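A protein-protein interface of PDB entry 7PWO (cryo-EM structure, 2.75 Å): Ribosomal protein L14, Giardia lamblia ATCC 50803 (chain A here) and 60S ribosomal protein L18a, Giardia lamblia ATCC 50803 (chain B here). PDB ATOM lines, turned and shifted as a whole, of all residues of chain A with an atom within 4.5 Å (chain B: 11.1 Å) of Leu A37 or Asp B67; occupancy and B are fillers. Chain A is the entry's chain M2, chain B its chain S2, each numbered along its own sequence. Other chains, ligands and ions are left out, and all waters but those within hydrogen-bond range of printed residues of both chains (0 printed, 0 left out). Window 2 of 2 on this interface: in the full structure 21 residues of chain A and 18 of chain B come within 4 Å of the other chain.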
ATOM      1  N   ILE A  27      37.141 -25.820  22.787  1.00  0.00           N
ATOM      2  CA  ILE A  27      35.792 -25.261  22.895  1.00  0.00           C
ATOM      3  C   ILE A  27      35.008 -25.551  21.620  1.00  0.00           C
ATOM      4  O   ILE A  27      35.479 -25.277  20.511  1.00  0.00           O
ATOM      5  CB  ILE A  27      35.839 -23.750  23.179  1.00  0.00           C
ATOM      6  CG1 ILE A  27      36.496 -23.457  24.525  1.00  0.00           C
ATOM      7  CG2 ILE A  27      34.458 -23.131  23.120  1.00  0.00           C
ATOM      8  CD1 ILE A  27      36.793 -22.017  24.732  1.00  0.00           C
ATOM      9  N   VAL A  28      33.799 -26.090  21.772  1.00  0.00           N
ATOM     10  CA  VAL A  28      32.936 -26.354  20.634  1.00  0.00           C
ATOM     11  C   VAL A  28      31.757 -25.386  20.548  1.00  0.00           C
ATOM     12  O   VAL A  28      31.265 -25.140  19.441  1.00  0.00           O
ATOM     13  CB  VAL A  28      32.439 -27.817  20.625  1.00  0.00           C
ATOM     14  CG1 VAL A  28      33.613 -28.791  20.501  1.00  0.00           C
ATOM     15  CG2 VAL A  28      31.625 -28.128  21.850  1.00  0.00           C
ATOM     16  N   ASP A  29      31.285 -24.821  21.664  1.00  0.00           N
ATOM     17  CA  ASP A  29      30.172 -23.880  21.548  1.00  0.00           C
ATOM     18  C   ASP A  29      30.140 -22.925  22.740  1.00  0.00           C
ATOM     19  O   ASP A  29      30.780 -23.153  23.766  1.00  0.00           O
ATOM     20  CB  ASP A  29      28.836 -24.606  21.399  1.00  0.00           C
ATOM     21  CG  ASP A  29      27.844 -23.812  20.567  1.00  0.00           C
ATOM     22  OD1 ASP A  29      28.122 -22.628  20.294  1.00  0.00           O
ATOM     23  OD2 ASP A  29      26.790 -24.358  20.185  1.00  0.00           O
ATOM     24  N   LEU A  31      27.708 -20.666  25.221  1.00  0.00           N
ATOM     25  CA  LEU A  31      26.336 -20.514  25.697  1.00  0.00           C
ATOM     26  C   LEU A  31      26.007 -19.051  25.967  1.00  0.00           C
ATOM     27  O   LEU A  31      25.068 -18.494  25.391  1.00  0.00           O
ATOM     28  CB  LEU A  31      26.120 -21.348  26.962  1.00  0.00           C
ATOM     29  CG  LEU A  31      25.743 -22.823  26.847  1.00  0.00           C
ATOM     30  CD1 LEU A  31      26.831 -23.618  26.154  1.00  0.00           C
ATOM     31  CD2 LEU A  31      25.437 -23.393  28.215  1.00  0.00           C
ATOM     32  N   VAL A  36      30.579 -22.414  28.476  1.00  0.00           N
ATOM     33  CA  VAL A  36      30.886 -22.961  27.166  1.00  0.00           C
ATOM     34  C   VAL A  36      30.616 -24.455  27.165  1.00  0.00           C
ATOM     35  O   VAL A  36      30.560 -25.107  28.210  1.00  0.00           O
ATOM     36  CB  VAL A  36      32.346 -22.681  26.729  1.00  0.00           C
ATOM     37  CG1 VAL A  36      32.602 -21.201  26.609  1.00  0.00           C
ATOM     38  CG2 VAL A  36      33.311 -23.270  27.725  1.00  0.00           C
ATOM     39  N   LEU A  37      30.433 -24.985  25.964  1.00  0.00           N
ATOM     40  CA  LEU A  37      30.449 -26.415  25.711  1.00  0.00           C
ATOM     41  C   LEU A  37      31.835 -26.765  25.190  1.00  0.00           C
ATOM     42  O   LEU A  37      32.278 -26.201  24.182  1.00  0.00           O
ATOM     43  CB  LEU A  37      29.372 -26.801  24.700  1.00  0.00           C
ATOM     44  CG  LEU A  37      29.126 -28.283  24.412  1.00  0.00           C
ATOM     45  CD1 LEU A  37      28.776 -29.035  25.679  1.00  0.00           C
ATOM     46  CD2 LEU A  37      28.050 -28.460  23.360  1.00  0.00           C
ATOM     47  N   ILE A  38      32.519 -27.671  25.890  1.00  0.00           N
ATOM     48  CA  ILE A  38      33.872 -28.094  25.559  1.00  0.00           C
ATOM     49  C   ILE A  38      33.898 -29.588  25.276  1.00  0.00           C
ATOM     50  O   ILE A  38      33.032 -30.352  25.712  1.00  0.00           O
ATOM     51  CB  ILE A  38      34.892 -27.766  26.665  1.00  0.00           C
ATOM     52  CG1 ILE A  38      34.533 -28.506  27.954  1.00  0.00           C
ATOM     53  CG2 ILE A  38      34.990 -26.282  26.881  1.00  0.00           C
ATOM     54  CD1 ILE A  38      35.602 -28.428  29.001  1.00  0.00           C
ATOM     55  N   ARG A  47      32.177 -34.538  26.525  1.00  0.00           N
ATOM     56  CA  ARG A  47      31.617 -33.271  26.070  1.00  0.00           C
ATOM     57  C   ARG A  47      30.675 -32.711  27.119  1.00  0.00           C
ATOM     58  O   ARG A  47      29.770 -33.407  27.585  1.00  0.00           O
ATOM     59  CB  ARG A  47      30.878 -33.449  24.749  1.00  0.00           C
ATOM     60  CG  ARG A  47      30.267 -32.170  24.241  1.00  0.00           C
ATOM     61  CD  ARG A  47      29.620 -32.383  22.900  1.00  0.00           C
ATOM     62  NE  ARG A  47      30.618 -32.389  21.834  1.00  0.00           N
ATOM     63  CZ  ARG A  47      30.344 -32.164  20.555  1.00  0.00           C
ATOM     64  NH1 ARG A  47      29.102 -31.909  20.175  1.00  0.00           N
ATOM     65  NH2 ARG A  47      31.316 -32.196  19.656  1.00  0.00           N
ATOM     66  N   GLN A  48      30.874 -31.449  27.486  1.00  0.00           N
ATOM     67  CA  GLN A  48      30.169 -30.970  28.667  1.00  0.00           C
ATOM     68  C   GLN A  48      30.211 -29.453  28.749  1.00  0.00           C
ATOM     69  O   GLN A  48      31.030 -28.799  28.102  1.00  0.00           O
ATOM     70  CB  GLN A  48      30.766 -31.587  29.937  1.00  0.00           C
ATOM     71  CG  GLN A  48      32.189 -31.146  30.212  1.00  0.00           C
ATOM     72  CD  GLN A  48      32.930 -32.093  31.129  1.00  0.00           C
ATOM     73  OE1 GLN A  48      33.004 -31.879  32.334  1.00  0.00           O
ATOM     74  NE2 GLN A  48      33.477 -33.155  30.560  1.00  0.00           N
ATOM     75  N   VAL A  49      29.333 -28.909  29.579  1.00  0.00           N
ATOM     76  CA  VAL A  49      29.284 -27.476  29.834  1.00  0.00           C
ATOM     77  C   VAL A  49      30.135 -27.146  31.053  1.00  0.00           C
ATOM     78  O   VAL A  49      29.902 -27.663  32.149  1.00  0.00           O
ATOM     79  CB  VAL A  49      27.842 -26.991  30.029  1.00  0.00           C
ATOM     80  CG1 VAL A  49      27.839 -25.532  30.403  1.00  0.00           C
ATOM     81  CG2 VAL A  49      27.063 -27.181  28.752  1.00  0.00           C
ATOM     82  N   GLU B  63      15.464 -39.262  30.440  1.00  0.00           N
ATOM     83  CA  GLU B  63      16.801 -38.762  30.173  1.00  0.00           C
ATOM     84  C   GLU B  63      16.873 -38.185  28.761  1.00  0.00           C
ATOM     85  O   GLU B  63      16.113 -38.565  27.869  1.00  0.00           O
ATOM     86  CB  GLU B  63      17.829 -39.876  30.346  1.00  0.00           C
ATOM     87  CG  GLU B  63      18.145 -40.196  31.799  1.00  0.00           C
ATOM     88  CD  GLU B  63      17.426 -41.427  32.301  1.00  0.00           C
ATOM     89  OE1 GLU B  63      16.701 -42.056  31.511  1.00  0.00           O
ATOM     90  OE2 GLU B  63      17.586 -41.770  33.488  1.00  0.00           O
ATOM     91  N   GLU B  64      17.809 -37.263  28.562  1.00  0.00           N
ATOM     92  CA  GLU B  64      17.861 -36.465  27.349  1.00  0.00           C
ATOM     93  C   GLU B  64      19.273 -36.435  26.782  1.00  0.00           C
ATOM     94  O   GLU B  64      20.262 -36.477  27.518  1.00  0.00           O
ATOM     95  CB  GLU B  64      17.388 -35.048  27.626  1.00  0.00           C
ATOM     96  CG  GLU B  64      15.879 -34.899  27.608  1.00  0.00           C
ATOM     97  CD  GLU B  64      15.425 -33.589  28.198  1.00  0.00           C
ATOM     98  OE1 GLU B  64      15.004 -33.579  29.368  1.00  0.00           O
ATOM     99  OE2 GLU B  64      15.492 -32.571  27.489  1.00  0.00           O
ATOM    100  N   ASN B  65      19.352 -36.359  25.457  1.00  0.00           N
ATOM    101  CA  ASN B  65      20.623 -36.214  24.772  1.00  0.00           C
ATOM    102  C   ASN B  65      21.071 -34.761  24.818  1.00  0.00           C
ATOM    103  O   ASN B  65      20.259 -33.840  24.909  1.00  0.00           O
ATOM    104  CB  ASN B  65      20.504 -36.684  23.320  1.00  0.00           C
ATOM    105  CG  ASN B  65      21.761 -36.426  22.509  1.00  0.00           C
ATOM    106  OD1 ASN B  65      22.001 -35.315  22.039  1.00  0.00           O
ATOM    107  ND2 ASN B  65      22.568 -37.463  22.336  1.00  0.00           N
ATOM    108  N   GLY B  66      22.384 -34.562  24.765  1.00  0.00           N
ATOM    109  CA  GLY B  66      22.927 -33.221  24.780  1.00  0.00           C
ATOM    110  C   GLY B  66      23.774 -32.849  23.581  1.00  0.00           C
ATOM    111  O   GLY B  66      23.348 -32.967  22.430  1.00  0.00           O
ATOM    112  N   ASP B  67      24.964 -32.328  23.869  1.00  0.00           N
ATOM    113  CA  ASP B  67      26.054 -32.152  22.916  1.00  0.00           C
ATOM    114  C   ASP B  67      25.835 -31.003  21.939  1.00  0.00           C
ATOM    115  O   ASP B  67      26.774 -30.610  21.242  1.00  0.00           O
ATOM    116  CB  ASP B  67      26.290 -33.461  22.160  1.00  0.00           C
ATOM    117  CG  ASP B  67      26.416 -34.645  23.091  1.00  0.00           C
ATOM    118  OD1 ASP B  67      27.407 -34.714  23.852  1.00  0.00           O
ATOM    119  OD2 ASP B  67      25.504 -35.496  23.085  1.00  0.00           O
ATOM    120  N   PHE B  68      24.637 -30.410  21.935  1.00  0.00           N
ATOM    121  CA  PHE B  68      24.332 -29.250  21.109  1.00  0.00           C
ATOM    122  C   PHE B  68      23.567 -28.238  21.954  1.00  0.00           C
ATOM    123  O   PHE B  68      22.869 -28.606  22.901  1.00  0.00           O
ATOM    124  CB  PHE B  68      23.525 -29.642  19.850  1.00  0.00           C
ATOM    125  CG  PHE B  68      24.159 -30.754  19.038  1.00  0.00           C
ATOM    126  CD1 PHE B  68      25.488 -30.685  18.650  1.00  0.00           C
ATOM    127  CD2 PHE B  68      23.431 -31.887  18.706  1.00  0.00           C
ATOM    128  CE1 PHE B  68      26.077 -31.711  17.928  1.00  0.00           C
ATOM    129  CE2 PHE B  68      24.007 -32.921  17.987  1.00  0.00           C
ATOM    130  CZ  PHE B  68      25.337 -32.834  17.595  1.00  0.00           C
ATOM    131  N   VAL B  69      23.695 -26.957  21.598  1.00  0.00           N
ATOM    132  CA  VAL B  69      23.182 -25.849  22.401  1.00  0.00           C
ATOM    133  C   VAL B  69      21.916 -25.313  21.758  1.00  0.00           C
ATOM    134  O   VAL B  69      21.902 -24.992  20.563  1.00  0.00           O
ATOM    135  CB  VAL B  69      24.227 -24.732  22.549  1.00  0.00           C
ATOM    136  CG1 VAL B  69      23.581 -23.458  23.112  1.00  0.00           C
ATOM    137  CG2 VAL B  69      25.365 -25.197  23.411  1.00  0.00           C
ATOM    138  N   LYS B  70      20.862 -25.183  22.557  1.00  0.00           N
ATOM    139  CA  LYS B  70      19.527 -24.885  22.066  1.00  0.00           C
ATOM    140  C   LYS B  70      18.997 -23.653  22.782  1.00  0.00           C
ATOM    141  O   LYS B  70      19.545 -23.219  23.797  1.00  0.00           O
ATOM    142  CB  LYS B  70      18.601 -26.093  22.279  1.00  0.00           C
ATOM    143  CG  LYS B  70      19.362 -27.415  22.236  1.00  0.00           C
ATOM    144  CD  LYS B  70      18.527 -28.612  21.817  1.00  0.00           C
ATOM    145  CE  LYS B  70      17.701 -29.137  22.979  1.00  0.00           C
ATOM    146  NZ  LYS B  70      16.912 -30.357  22.646  1.00  0.00           N
ATOM    147  N   PHE B  72      15.694 -22.157  24.749  1.00  0.00           N
ATOM    148  CA  PHE B  72      14.458 -22.519  25.427  1.00  0.00           C
ATOM    149  C   PHE B  72      13.745 -21.269  25.907  1.00  0.00           C
ATOM    150  O   PHE B  72      14.333 -20.442  26.613  1.00  0.00           O
ATOM    151  CB  PHE B  72      14.723 -23.472  26.585  1.00  0.00           C
ATOM    152  CG  PHE B  72      15.199 -24.805  26.143  1.00  0.00           C
ATOM    153  CD1 PHE B  72      16.536 -25.033  25.919  1.00  0.00           C
ATOM    154  CD2 PHE B  72      14.300 -25.816  25.886  1.00  0.00           C
ATOM    155  CE1 PHE B  72      16.969 -26.248  25.488  1.00  0.00           C
ATOM    156  CE2 PHE B  72      14.730 -27.033  25.446  1.00  0.00           C
ATOM    157  CZ  PHE B  72      16.065 -27.252  25.253  1.00  0.00           C
ATOM    158  N   ARG B  92      19.905 -20.188  26.861  1.00  0.00           N
ATOM    159  CA  ARG B  92      20.638 -21.110  26.001  1.00  0.00           C
ATOM    160  C   ARG B  92      21.257 -22.182  26.882  1.00  0.00           C
ATOM    161  O   ARG B  92      22.180 -21.902  27.653  1.00  0.00           O
ATOM    162  CB  ARG B  92      21.705 -20.400  25.178  1.00  0.00           C
ATOM    163  CG  ARG B  92      21.252 -20.064  23.787  1.00  0.00           C
ATOM    164  CD  ARG B  92      22.218 -19.132  23.077  1.00  0.00           C
ATOM    165  NE  ARG B  92      23.350 -19.829  22.476  1.00  0.00           N
ATOM    166  CZ  ARG B  92      23.306 -20.463  21.310  1.00  0.00           C
ATOM    167  NH1 ARG B  92      22.178 -20.503  20.621  1.00  0.00           N
ATOM    168  NH2 ARG B  92      24.390 -21.059  20.833  1.00  0.00           N
ATOM    169  N   GLU B  93      20.750 -23.406  26.763  1.00  0.00           N
ATOM    170  CA  GLU B  93      21.269 -24.540  27.505  1.00  0.00           C
ATOM    171  C   GLU B  93      21.218 -25.768  26.615  1.00  0.00           C
ATOM    172  O   GLU B  93      20.811 -25.708  25.454  1.00  0.00           O
ATOM    173  CB  GLU B  93      20.492 -24.774  28.811  1.00  0.00           C
ATOM    174  CG  GLU B  93      21.029 -24.012  30.013  1.00  0.00           C
ATOM    175  CD  GLU B  93      22.369 -24.542  30.509  1.00  0.00           C
ATOM    176  OE1 GLU B  93      23.103 -23.784  31.180  1.00  0.00           O
ATOM    177  OE2 GLU B  93      22.689 -25.711  30.237  1.00  0.00           O
ATOM    178  N   THR B  94      21.643 -26.892  27.173  1.00  0.00           N
ATOM    179  CA  THR B  94      21.750 -28.109  26.387  1.00  0.00           C
ATOM    180  C   THR B  94      20.500 -28.976  26.480  1.00  0.00           C
ATOM    181  O   THR B  94      20.076 -29.555  25.475  1.00  0.00           O
ATOM    182  CB  THR B  94      22.988 -28.891  26.826  1.00  0.00           C
ATOM    183  OG1 THR B  94      24.156 -28.088  26.619  1.00  0.00           O
ATOM    184  CG2 THR B  94      23.116 -30.132  26.043  1.00  0.00           C
ATOM    185  N   THR B  95      19.895 -29.062  27.663  1.00  0.00           N
ATOM    186  CA  THR B  95      18.686 -29.839  27.876  1.00  0.00           C
ATOM    187  C   THR B  95      17.659 -28.993  28.617  1.00  0.00           C
ATOM    188  O   THR B  95      17.985 -27.962  29.208  1.00  0.00           O
ATOM    189  CB  THR B  95      18.969 -31.130  28.658  1.00  0.00           C
ATOM    190  OG1 THR B  95      19.492 -30.812  29.951  1.00  0.00           O
ATOM    191  CG2 THR B  95      19.967 -31.983  27.926  1.00  0.00           C
ATOM    192  N   SER B  96      16.406 -29.448  28.569  1.00  0.00           N
ATOM    193  CA  SER B  96      15.313 -28.697  29.179  1.00  0.00           C
ATOM    194  C   SER B  96      15.485 -28.587  30.687  1.00  0.00           C
ATOM    195  O   SER B  96      15.203 -27.539  31.277  1.00  0.00           O
ATOM    196  CB  SER B  96      13.975 -29.349  28.845  1.00  0.00           C
ATOM    197  OG  SER B  96      13.714 -29.307  27.462  1.00  0.00           O
ATOM    198  N   ARG B  98      18.307 -28.513  32.414  1.00  0.00           N
ATOM    199  CA  ARG B  98      19.345 -27.525  32.693  1.00  0.00           C
ATOM    200  C   ARG B  98      18.850 -26.114  32.426  1.00  0.00           C
ATOM    201  O   ARG B  98      19.158 -25.182  33.180  1.00  0.00           O
ATOM    202  CB  ARG B  98      20.586 -27.815  31.856  1.00  0.00           C
ATOM    203  CG  ARG B  98      21.214 -29.136  32.141  1.00  0.00           C
ATOM    204  CD  ARG B  98      22.507 -29.306  31.370  1.00  0.00           C
ATOM    205  NE  ARG B  98      23.587 -28.500  31.930  1.00  0.00           N
ATOM    206  CZ  ARG B  98      24.411 -28.951  32.866  1.00  0.00           C
ATOM    207  NH1 ARG B  98      24.257 -30.179  33.330  1.00  0.00           N
ATOM    208  NH2 ARG B  98      25.381 -28.189  33.337  1.00  0.00           N
ATOM    209  N   GLU B 125      11.269 -25.094  22.610  1.00  0.00           N
ATOM    210  CA  GLU B 125      12.458 -24.720  21.856  1.00  0.00           C
ATOM    211  C   GLU B 125      12.146 -23.619  20.852  1.00  0.00           C
ATOM    212  O   GLU B 125      11.128 -23.664  20.157  1.00  0.00           O
ATOM    213  CB  GLU B 125      13.032 -25.935  21.136  1.00  0.00           C
ATOM    214  CG  GLU B 125      13.479 -27.040  22.066  1.00  0.00           C
ATOM    215  CD  GLU B 125      14.397 -28.046  21.382  1.00  0.00           C
ATOM    216  OE1 GLU B 125      13.933 -29.155  21.048  1.00  0.00           O
ATOM    217  OE2 GLU B 125      15.576 -27.712  21.157  1.00  0.00           O
ATOM    218  N   PHE B 139      24.222 -14.589  21.029  1.00  0.00           N
ATOM    219  CA  PHE B 139      25.016 -15.794  20.878  1.00  0.00           C
ATOM    220  C   PHE B 139      24.475 -16.731  19.810  1.00  0.00           C
ATOM    221  O   PHE B 139      25.096 -17.762  19.537  1.00  0.00           O
ATOM    222  CB  PHE B 139      25.095 -16.512  22.224  1.00  0.00           C
ATOM    223  CG  PHE B 139      25.855 -15.756  23.259  1.00  0.00           C
ATOM    224  CD1 PHE B 139      27.233 -15.811  23.292  1.00  0.00           C
ATOM    225  CD2 PHE B 139      25.199 -14.951  24.174  1.00  0.00           C
ATOM    226  CE1 PHE B 139      27.937 -15.107  24.227  1.00  0.00           C
ATOM    227  CE2 PHE B 139      25.905 -14.244  25.110  1.00  0.00           C
ATOM    228  CZ  PHE B 139      27.274 -14.323  25.136  1.00  0.00           C
ATOM    229  N   VAL B 144      30.983 -15.471  16.876  1.00  0.00           N
ATOM    230  CA  VAL B 144      30.951 -14.636  18.072  1.00  0.00           C
ATOM    231  C   VAL B 144      32.265 -14.795  18.830  1.00  0.00           C
ATOM    232  O   VAL B 144      32.718 -15.915  19.092  1.00  0.00           O
ATOM    233  CB  VAL B 144      29.728 -14.970  18.945  1.00  0.00           C
ATOM    234  CG1 VAL B 144      29.791 -16.381  19.501  1.00  0.00           C
ATOM    235  CG2 VAL B 144      29.587 -13.956  20.067  1.00  0.00           C
ATOM    236  N   PHE B 146      34.748 -12.947  22.088  1.00  0.00           N
ATOM    237  CA  PHE B 146      34.984 -11.980  23.140  1.00  0.00           C
ATOM    238  C   PHE B 146      36.214 -12.391  23.931  1.00  0.00           C
ATOM    239  O   PHE B 146      36.518 -13.585  24.030  1.00  0.00           O
ATOM    240  CB  PHE B 146      33.756 -11.811  24.052  1.00  0.00           C
ATOM    241  CG  PHE B 146      33.100 -13.105  24.473  1.00  0.00           C
ATOM    242  CD1 PHE B 146      32.176 -13.727  23.643  1.00  0.00           C
ATOM    243  CD2 PHE B 146      33.362 -13.667  25.708  1.00  0.00           C
ATOM    244  CE1 PHE B 146      31.556 -14.900  24.023  1.00  0.00           C
ATOM    245  CE2 PHE B 146      32.741 -14.847  26.093  1.00  0.00           C
ATOM    246  CZ  PHE B 146      31.840 -15.461  25.254  1.00  0.00           C
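O of Asp B67 lies within hydrogen-bond range of NH1 of Arg A47 (2.9 Å).
OD2 of Asp A29 touches CB of Val B69, at 3.5 Å.
Leu A31 touches Val B69 (CD1 to CG2, 3.5 Å).
Leu A31 touches Arg B92.
Leu A31 touches Glu B93.
Leu A31 touches Phe B139 (O to CG, 3.6 Å).
Leu A37 touches Asp B67 (CD2 to O, 3.3 Å).
CE1 of Phe B68 touches NH1 of Arg A47, at 3.8 Å.
Val A49 touches Thr B94 (CG2 to OG1, 3.7 Å).
Val A28 touches none of the printed residues of chain B.
Asp A29 touches just one residue of chain B: Val B69.
Printed residues of chain B within 4 Å of Leu A31: Val B69 (3.5 Å), Arg B92 (3.6 Å), Glu B93 (3.8 Å) and Phe B139 (3.6 Å).
Val A36 touches none of the printed residues of chain B.
Of chain B, only Asp B67 comes within 4 Å of Leu A37.
Val A49 touches just one residue of chain B: Thr B94.
Asp B67 touches just these residues of chain A: Leu A37 and Arg A47.
Of the printed residues of chain A, Val B69 touches Asp A29 (3.5 Å) and Leu A31 (3.5 Å).
Printed residues of chain A within 4 Å of Arg B92: Leu A31.
Of the printed residues of chain A, Glu B93 touches Leu A31 (3.8 Å).
Val B144 touches none of the printed residues of chain A.
The nearest printed residue of chain A that does not touch Asp B67 is Val A28 (5.5 Å).
The nearest printed residue of chain A that does not touch Val B69 is Leu A37 (4.2 Å).
The backbone NH (N) of Leu A37 sits at hydrogen-bond distance from the backbone carbonyl oxygen (O) of Asp A29 (2.9 Å).
The side-chain carboxylate (OE2) of Glu B93 lies within salt-bridge range of the guanidinium group (NE) of Arg B98, 3.4 Å away.
O of Leu A37 lies within hydrogen-bond range of N of Val A28 (2.9 Å).
The backbone NH of Lys B70 lies within hydrogen-bond range of the backbone carbonyl oxygen of Glu B93, at 2.9 Å.
Printed residues of chain B that touch a printed residue of chain A: Asp B67, Phe B68, Val B69, Arg B92, Glu B93, Thr B94 and Phe B139.
Hydrophobic or aromatic side chains of chain B that line the printed part of chain A: Phe B68, Val B69 and Phe B139.
Among the printed residues, no Asp or Glu carboxylate lies within 4 Å of a Lys or Arg side-chain nitrogen of the other chain.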
